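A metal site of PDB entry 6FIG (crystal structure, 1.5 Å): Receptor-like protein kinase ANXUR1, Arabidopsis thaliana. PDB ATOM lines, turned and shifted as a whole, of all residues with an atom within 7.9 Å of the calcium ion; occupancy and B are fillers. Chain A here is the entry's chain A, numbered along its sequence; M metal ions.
The backbone carbonyl oxygen of Glu 23 is in hydrogen-bond range of the backbone NH of Ser 7 (2.8 Å). SG of Cys 8 lies close to OD2 of Asp 25. N of Asn 154 lies within hydrogen-bond range of O of Tyr 79, at 3.0 Å. ND2 of Asn 154 lies within hydrogen-bond range of OH of Tyr 85. O of Ser 7 is in hydrogen-bond range of OG1 of Thr 10 (2.7 Å). The backbone NH (N) of Ala 55 lies close to the backbone carbonyl oxygen (O) of Cys 8 (3.4 Å). The side-chain amide nitrogen (ND2) of Asn 154 lies within hydrogen-bond range of the backbone carbonyl oxygen (O) of Tyr 52.
Within 4 Å of the calcium ion: Ser 7, Cys 8, Pro 51, Thr 54 and Asn 154.
The calcium ion is bound by OG1 of Thr 54 (2.4 Å). O of Thr 54 is bound to the calcium ion (2.4 Å). The calcium ion is bound by the backbone carbonyl oxygen (O) of Asn 154 (2.4 Å). The backbone carbonyl oxygen (O) of Pro 51 is bound to the calcium ion, at 2.5 Å. O of Cys 8 is bound to the calcium ion. The side-chain hydroxyl (OG) of Ser 7 is bound to the calcium ion (2.6 Å).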
ATOM      1  N   LEU A   6     -14.281  -8.658  -4.615  1.00  0.00           N
ATOM      2  CA  LEU A   6     -14.505  -7.923  -5.848  1.00  0.00           C
ATOM      3  C   LEU A   6     -14.890  -8.887  -6.953  1.00  0.00           C
ATOM      4  O   LEU A   6     -14.143  -9.823  -7.255  1.00  0.00           O
ATOM      5  CB  LEU A   6     -13.250  -7.170  -6.255  1.00  0.00           C
ATOM      6  CG  LEU A   6     -12.571  -6.307  -5.200  1.00  0.00           C
ATOM      7  CD1 LEU A   6     -11.337  -5.653  -5.782  1.00  0.00           C
ATOM      8  CD2 LEU A   6     -13.551  -5.283  -4.640  1.00  0.00           C
ATOM      9  N   SER A   7     -16.066  -8.678  -7.543  1.00  0.00           N
ATOM     10  CA  SER A   7     -16.461  -9.468  -8.700  1.00  0.00           C
ATOM     11  C   SER A   7     -16.099  -8.638  -9.905  1.00  0.00           C
ATOM     12  O   SER A   7     -16.725  -7.595 -10.171  1.00  0.00           O
ATOM     13  CB  SER A   7     -17.935  -9.827  -8.704  1.00  0.00           C
ATOM     14  OG  SER A   7     -18.204 -10.662  -9.834  1.00  0.00           O
ATOM     15  N   CYS A   8     -15.058  -9.049 -10.609  1.00  0.00           N
ATOM     16  CA  CYS A   8     -14.496  -8.261 -11.675  1.00  0.00           C
ATOM     17  C   CYS A   8     -15.451  -8.292 -12.869  1.00  0.00           C
ATOM     18  O   CYS A   8     -16.006  -9.349 -13.182  1.00  0.00           O
ATOM     19  CB  CYS A   8     -13.127  -8.799 -12.036  1.00  0.00           C
ATOM     20  SG  CYS A   8     -12.097  -8.874 -10.567  1.00  0.00           S
ATOM     21  N   GLY A   9     -15.664  -7.134 -13.461  1.00  0.00           N
ATOM     22  CA  GLY A   9     -16.550  -6.993 -14.607  1.00  0.00           C
ATOM     23  C   GLY A   9     -18.013  -6.721 -14.288  1.00  0.00           C
ATOM     24  O   GLY A   9     -18.843  -6.700 -15.198  1.00  0.00           O
ATOM     25  N   THR A  10     -18.336  -6.507 -13.019  1.00  0.00           N
ATOM     26  CA  THR A  10     -19.702  -6.162 -12.612  1.00  0.00           C
ATOM     27  C   THR A  10     -19.804  -4.680 -12.367  1.00  0.00           C
ATOM     28  O   THR A  10     -18.797  -3.983 -12.185  1.00  0.00           O
ATOM     29  CB  THR A  10     -20.136  -6.912 -11.322  1.00  0.00           C
ATOM     30  OG1 THR A  10     -19.235  -6.616 -10.244  1.00  0.00           O
ATOM     31  CG2 THR A  10     -20.179  -8.418 -11.534  1.00  0.00           C
ATOM     32  N   SER A  14     -23.438  -7.802  -5.798  1.00  0.00           N
ATOM     33  CA  SER A  14     -23.958  -9.145  -6.047  1.00  0.00           C
ATOM     34  C   SER A  14     -23.670 -10.025  -4.831  1.00  0.00           C
ATOM     35  O   SER A  14     -22.885  -9.641  -3.973  1.00  0.00           O
ATOM     36  CB  SER A  14     -23.334  -9.734  -7.309  1.00  0.00           C
ATOM     37  OG  SER A  14     -21.919  -9.798  -7.239  1.00  0.00           O
ATOM     38  N   TRP A  22     -20.476  -9.495  -2.754  1.00  0.00           N
ATOM     39  CA  TRP A  22     -19.437  -9.066  -3.692  1.00  0.00           C
ATOM     40  C   TRP A  22     -19.773  -7.674  -4.221  1.00  0.00           C
ATOM     41  O   TRP A  22     -20.952  -7.282  -4.264  1.00  0.00           O
ATOM     42  CB  TRP A  22     -19.358 -10.028  -4.877  1.00  0.00           C
ATOM     43  CG  TRP A  22     -18.935 -11.416  -4.556  1.00  0.00           C
ATOM     44  CD1 TRP A  22     -19.701 -12.400  -4.018  1.00  0.00           C
ATOM     45  CD2 TRP A  22     -17.648 -12.004  -4.798  1.00  0.00           C
ATOM     46  NE1 TRP A  22     -18.980 -13.570  -3.914  1.00  0.00           N
ATOM     47  CE2 TRP A  22     -17.716 -13.341  -4.372  1.00  0.00           C
ATOM     48  CE3 TRP A  22     -16.451 -11.517  -5.309  1.00  0.00           C
ATOM     49  CZ2 TRP A  22     -16.625 -14.221  -4.462  1.00  0.00           C
ATOM     50  CZ3 TRP A  22     -15.365 -12.384  -5.400  1.00  0.00           C
ATOM     51  CH2 TRP A  22     -15.449 -13.710  -4.959  1.00  0.00           C
ATOM     52  N   GLU A  23     -18.741  -6.941  -4.609  1.00  0.00           N
ATOM     53  CA  GLU A  23     -18.892  -5.610  -5.181  1.00  0.00           C
ATOM     54  C   GLU A  23     -18.065  -5.466  -6.449  1.00  0.00           C
ATOM     55  O   GLU A  23     -17.161  -6.262  -6.687  1.00  0.00           O
ATOM     56  CB  GLU A  23     -18.487  -4.533  -4.166  1.00  0.00           C
ATOM     57  CG  GLU A  23     -17.003  -4.469  -3.826  1.00  0.00           C
ATOM     58  CD  GLU A  23     -16.690  -3.350  -2.854  1.00  0.00           C
ATOM     59  OE1 GLU A  23     -16.932  -2.180  -3.173  1.00  0.00           O
ATOM     60  OE2 GLU A  23     -16.211  -3.644  -1.747  1.00  0.00           O
ATOM     61  N   ASP A  25     -15.193  -4.307  -9.036  1.00  0.00           N
ATOM     62  CA  ASP A  25     -13.754  -4.096  -8.861  1.00  0.00           C
ATOM     63  C   ASP A  25     -13.277  -2.708  -9.274  1.00  0.00           C
ATOM     64  O   ASP A  25     -12.125  -2.352  -9.024  1.00  0.00           O
ATOM     65  CB  ASP A  25     -12.960  -5.165  -9.612  1.00  0.00           C
ATOM     66  CG  ASP A  25     -13.103  -5.072 -11.119  1.00  0.00           C
ATOM     67  OD1 ASP A  25     -14.151  -4.602 -11.621  1.00  0.00           O
ATOM     68  OD2 ASP A  25     -12.176  -5.508 -11.843  1.00  0.00           O
ATOM     69  N   ALA A  37     -16.553  -8.190 -19.377  1.00  0.00           N
ATOM     70  CA  ALA A  37     -17.038  -9.231 -20.270  1.00  0.00           C
ATOM     71  C   ALA A  37     -17.895 -10.204 -19.500  1.00  0.00           C
ATOM     72  O   ALA A  37     -17.655 -10.472 -18.330  1.00  0.00           O
ATOM     73  CB  ALA A  37     -15.883  -9.952 -20.934  1.00  0.00           C
ATOM     74  N   THR A  49     -23.524 -17.847 -10.318  1.00  0.00           N
ATOM     75  CA  THR A  49     -23.018 -16.983 -11.397  1.00  0.00           C
ATOM     76  C   THR A  49     -22.050 -15.913 -10.833  1.00  0.00           C
ATOM     77  O   THR A  49     -21.428 -15.190 -11.604  1.00  0.00           O
ATOM     78  CB  THR A  49     -24.134 -16.273 -12.185  1.00  0.00           C
ATOM     79  OG1 THR A  49     -24.844 -15.374 -11.331  1.00  0.00           O
ATOM     80  CG2 THR A  49     -25.114 -17.271 -12.819  1.00  0.00           C
ATOM     81  N   VAL A  50     -21.944 -15.803  -9.500  1.00  0.00           N
ATOM     82  CA  VAL A  50     -21.141 -14.780  -8.822  1.00  0.00           C
ATOM     83  C   VAL A  50     -19.921 -15.462  -8.168  1.00  0.00           C
ATOM     84  O   VAL A  50     -20.114 -16.368  -7.358  1.00  0.00           O
ATOM     85  CB  VAL A  50     -21.976 -14.109  -7.712  1.00  0.00           C
ATOM     86  CG1 VAL A  50     -21.161 -13.078  -6.940  1.00  0.00           C
ATOM     87  CG2 VAL A  50     -23.250 -13.471  -8.289  1.00  0.00           C
ATOM     88  N   PRO A  51     -18.669 -15.083  -8.477  1.00  0.00           N
ATOM     89  CA  PRO A  51     -18.266 -14.013  -9.400  1.00  0.00           C
ATOM     90  C   PRO A  51     -18.013 -14.511 -10.833  1.00  0.00           C
ATOM     91  O   PRO A  51     -17.631 -13.710 -11.690  1.00  0.00           O
ATOM     92  CB  PRO A  51     -16.935 -13.567  -8.799  1.00  0.00           C
ATOM     93  CG  PRO A  51     -16.338 -14.834  -8.309  1.00  0.00           C
ATOM     94  CD  PRO A  51     -17.496 -15.632  -7.760  1.00  0.00           C
ATOM     95  N   TYR A  52     -18.252 -15.794 -11.080  1.00  0.00           N
ATOM     96  CA  TYR A  52     -17.689 -16.488 -12.241  1.00  0.00           C
ATOM     97  C   TYR A  52     -18.158 -16.054 -13.634  1.00  0.00           C
ATOM     98  O   TYR A  52     -17.371 -16.157 -14.568  1.00  0.00           O
ATOM     99  CB  TYR A  52     -17.890 -18.009 -12.088  1.00  0.00           C
ATOM    100  CG  TYR A  52     -17.243 -18.573 -10.852  1.00  0.00           C
ATOM    101  CD1 TYR A  52     -15.860 -18.710 -10.767  1.00  0.00           C
ATOM    102  CD2 TYR A  52     -18.018 -18.969  -9.757  1.00  0.00           C
ATOM    103  CE1 TYR A  52     -15.262 -19.236  -9.629  1.00  0.00           C
ATOM    104  CE2 TYR A  52     -17.433 -19.493  -8.616  1.00  0.00           C
ATOM    105  CZ  TYR A  52     -16.058 -19.628  -8.560  1.00  0.00           C
ATOM    106  OH  TYR A  52     -15.463 -20.118  -7.431  1.00  0.00           O
ATOM    107  N   MET A  53     -19.399 -15.592 -13.792  1.00  0.00           N
ATOM    108  CA  MET A  53     -19.926 -15.305 -15.125  1.00  0.00           C
ATOM    109  C   MET A  53     -19.508 -13.949 -15.680  1.00  0.00           C
ATOM    110  O   MET A  53     -19.807 -13.640 -16.822  1.00  0.00           O
ATOM    111  CB  MET A  53     -21.457 -15.429 -15.155  1.00  0.00           C
ATOM    112  CG  MET A  53     -21.921 -16.870 -15.044  1.00  0.00           C
ATOM    113  SD  MET A  53     -21.423 -17.902 -16.444  1.00  0.00           S
ATOM    114  CE  MET A  53     -22.542 -17.341 -17.717  1.00  0.00           C
ATOM    115  N   THR A  54     -18.806 -13.145 -14.885  1.00  0.00           N
ATOM    116  CA  THR A  54     -18.338 -11.847 -15.318  1.00  0.00           C
ATOM    117  C   THR A  54     -16.841 -11.780 -15.126  1.00  0.00           C
ATOM    118  O   THR A  54     -16.331 -12.299 -14.155  1.00  0.00           O
ATOM    119  CB  THR A  54     -19.006 -10.742 -14.490  1.00  0.00           C
ATOM    120  OG1 THR A  54     -18.938 -11.107 -13.086  1.00  0.00           O
ATOM    121  CG2 THR A  54     -20.440 -10.581 -14.919  1.00  0.00           C
ATOM    122  N   ALA A  55     -16.150 -11.131 -16.056  1.00  0.00           N
ATOM    123  CA  ALA A  55     -14.705 -11.006 -15.986  1.00  0.00           C
ATOM    124  C   ALA A  55     -14.284  -9.633 -16.403  1.00  0.00           C
ATOM    125  O   ALA A  55     -15.036  -8.889 -17.028  1.00  0.00           O
ATOM    126  CB  ALA A  55     -14.046 -12.059 -16.861  1.00  0.00           C
ATOM    127  N   ARG A  56     -13.067  -9.289 -16.015  1.00  0.00           N
ATOM    128  CA  ARG A  56     -12.356  -8.188 -16.620  1.00  0.00           C
ATOM    129  C   ARG A  56     -11.270  -8.815 -17.497  1.00  0.00           C
ATOM    130  O   ARG A  56     -10.612  -9.759 -17.073  1.00  0.00           O
ATOM    131  CB  ARG A  56     -11.741  -7.303 -15.544  1.00  0.00           C
ATOM    132  CG  ARG A  56     -11.137  -6.042 -16.110  1.00  0.00           C
ATOM    133  CD  ARG A  56     -10.797  -5.031 -15.040  1.00  0.00           C
ATOM    134  NE  ARG A  56     -11.994  -4.484 -14.406  1.00  0.00           N
ATOM    135  CZ  ARG A  56     -12.792  -3.554 -14.925  1.00  0.00           C
ATOM    136  NH1 ARG A  56     -12.579  -3.022 -16.129  1.00  0.00           N
ATOM    137  NH2 ARG A  56     -13.836  -3.150 -14.200  1.00  0.00           N
ATOM    138  N   TYR A  79     -10.158 -15.782  -8.533  1.00  0.00           N
ATOM    139  CA  TYR A  79     -11.200 -16.652  -9.104  1.00  0.00           C
ATOM    140  C   TYR A  79     -11.134 -16.583 -10.621  1.00  0.00           C
ATOM    141  O   TYR A  79     -11.161 -15.486 -11.196  1.00  0.00           O
ATOM    142  CB  TYR A  79     -12.593 -16.190  -8.661  1.00  0.00           C
ATOM    143  CG  TYR A  79     -12.900 -16.344  -7.171  1.00  0.00           C
ATOM    144  CD1 TYR A  79     -12.243 -15.586  -6.208  1.00  0.00           C
ATOM    145  CD2 TYR A  79     -13.848 -17.270  -6.744  1.00  0.00           C
ATOM    146  CE1 TYR A  79     -12.513 -15.747  -4.851  1.00  0.00           C
ATOM    147  CE2 TYR A  79     -14.142 -17.434  -5.392  1.00  0.00           C
ATOM    148  CZ  TYR A  79     -13.483 -16.669  -4.450  1.00  0.00           C
ATOM    149  OH  TYR A  79     -13.801 -16.853  -3.117  1.00  0.00           O
ATOM    150  N   TYR A  85     -14.759 -14.928 -23.835  1.00  0.00           N
ATOM    151  CA  TYR A  85     -15.040 -13.550 -23.458  1.00  0.00           C
ATOM    152  C   TYR A  85     -14.724 -12.668 -24.649  1.00  0.00           C
ATOM    153  O   TYR A  85     -13.623 -12.784 -25.207  1.00  0.00           O
ATOM    154  CB  TYR A  85     -14.164 -13.155 -22.296  1.00  0.00           C
ATOM    155  CG  TYR A  85     -14.432 -13.933 -21.034  1.00  0.00           C
ATOM    156  CD1 TYR A  85     -15.584 -13.692 -20.285  1.00  0.00           C
ATOM    157  CD2 TYR A  85     -13.532 -14.873 -20.570  1.00  0.00           C
ATOM    158  CE1 TYR A  85     -15.840 -14.384 -19.122  1.00  0.00           C
ATOM    159  CE2 TYR A  85     -13.764 -15.577 -19.393  1.00  0.00           C
ATOM    160  CZ  TYR A  85     -14.921 -15.326 -18.669  1.00  0.00           C
ATOM    161  OH  TYR A  85     -15.150 -16.021 -17.489  1.00  0.00           O
ATOM    162  N   ILE A 153      -9.634 -12.080 -15.199  1.00  0.00           N
ATOM    163  CA  ILE A 153      -9.898 -12.331 -13.779  1.00  0.00           C
ATOM    164  C   ILE A 153     -11.408 -12.228 -13.567  1.00  0.00           C
ATOM    165  O   ILE A 153     -12.051 -11.331 -14.121  1.00  0.00           O
ATOM    166  CB  ILE A 153      -9.109 -11.335 -12.885  1.00  0.00           C
ATOM    167  CG1 ILE A 153      -9.320 -11.587 -11.383  1.00  0.00           C
ATOM    168  CG2 ILE A 153      -9.440  -9.884 -13.244  1.00  0.00           C
ATOM    169  CD1 ILE A 153      -8.697 -12.872 -10.866  1.00  0.00           C
ATOM    170  N   ASN A 154     -11.975 -13.135 -12.788  1.00  0.00           N
ATOM    171  CA  ASN A 154     -13.409 -13.089 -12.473  1.00  0.00           C
ATOM    172  C   ASN A 154     -13.709 -12.539 -11.088  1.00  0.00           C
ATOM    173  O   ASN A 154     -14.728 -11.861 -10.884  1.00  0.00           O
ATOM    174  CB  ASN A 154     -14.019 -14.464 -12.618  1.00  0.00           C
ATOM    175  CG  ASN A 154     -13.869 -15.000 -14.016  1.00  0.00           C
ATOM    176  OD1 ASN A 154     -12.864 -15.648 -14.321  1.00  0.00           O
ATOM    177  ND2 ASN A 154     -14.840 -14.732 -14.884  1.00  0.00           N
ATOM    178  N   GLY A 155     -12.811 -12.789 -10.144  1.00  0.00           N
ATOM    179  CA  GLY A 155     -13.003 -12.336  -8.787  1.00  0.00           C
ATOM    180  C   GLY A 155     -11.694 -12.212  -8.033  1.00  0.00           C
ATOM    181  O   GLY A 155     -10.752 -12.963  -8.275  1.00  0.00           O
ATOM    182  N   ILE A 156     -11.667 -11.253  -7.118  1.00  0.00           N
ATOM    183  CA  ILE A 156     -10.512 -11.045  -6.223  1.00  0.00           C
ATOM    184  C   ILE A 156     -11.028 -10.884  -4.799  1.00  0.00           C
ATOM    185  O   ILE A 156     -11.894 -10.073  -4.571  1.00  0.00           O
ATOM    186  CB  ILE A 156      -9.686  -9.814  -6.635  1.00  0.00           C
ATOM    187  CG1 ILE A 156      -9.146  -9.972  -8.056  1.00  0.00           C
ATOM    188  CG2 ILE A 156      -8.543  -9.586  -5.661  1.00  0.00           C
ATOM    189  CD1 ILE A 156      -8.470  -8.734  -8.614  1.00  0.00           C
HETATM  190 CA    CA M   1     -16.840 -11.405 -11.971  1.00  0.00          CA
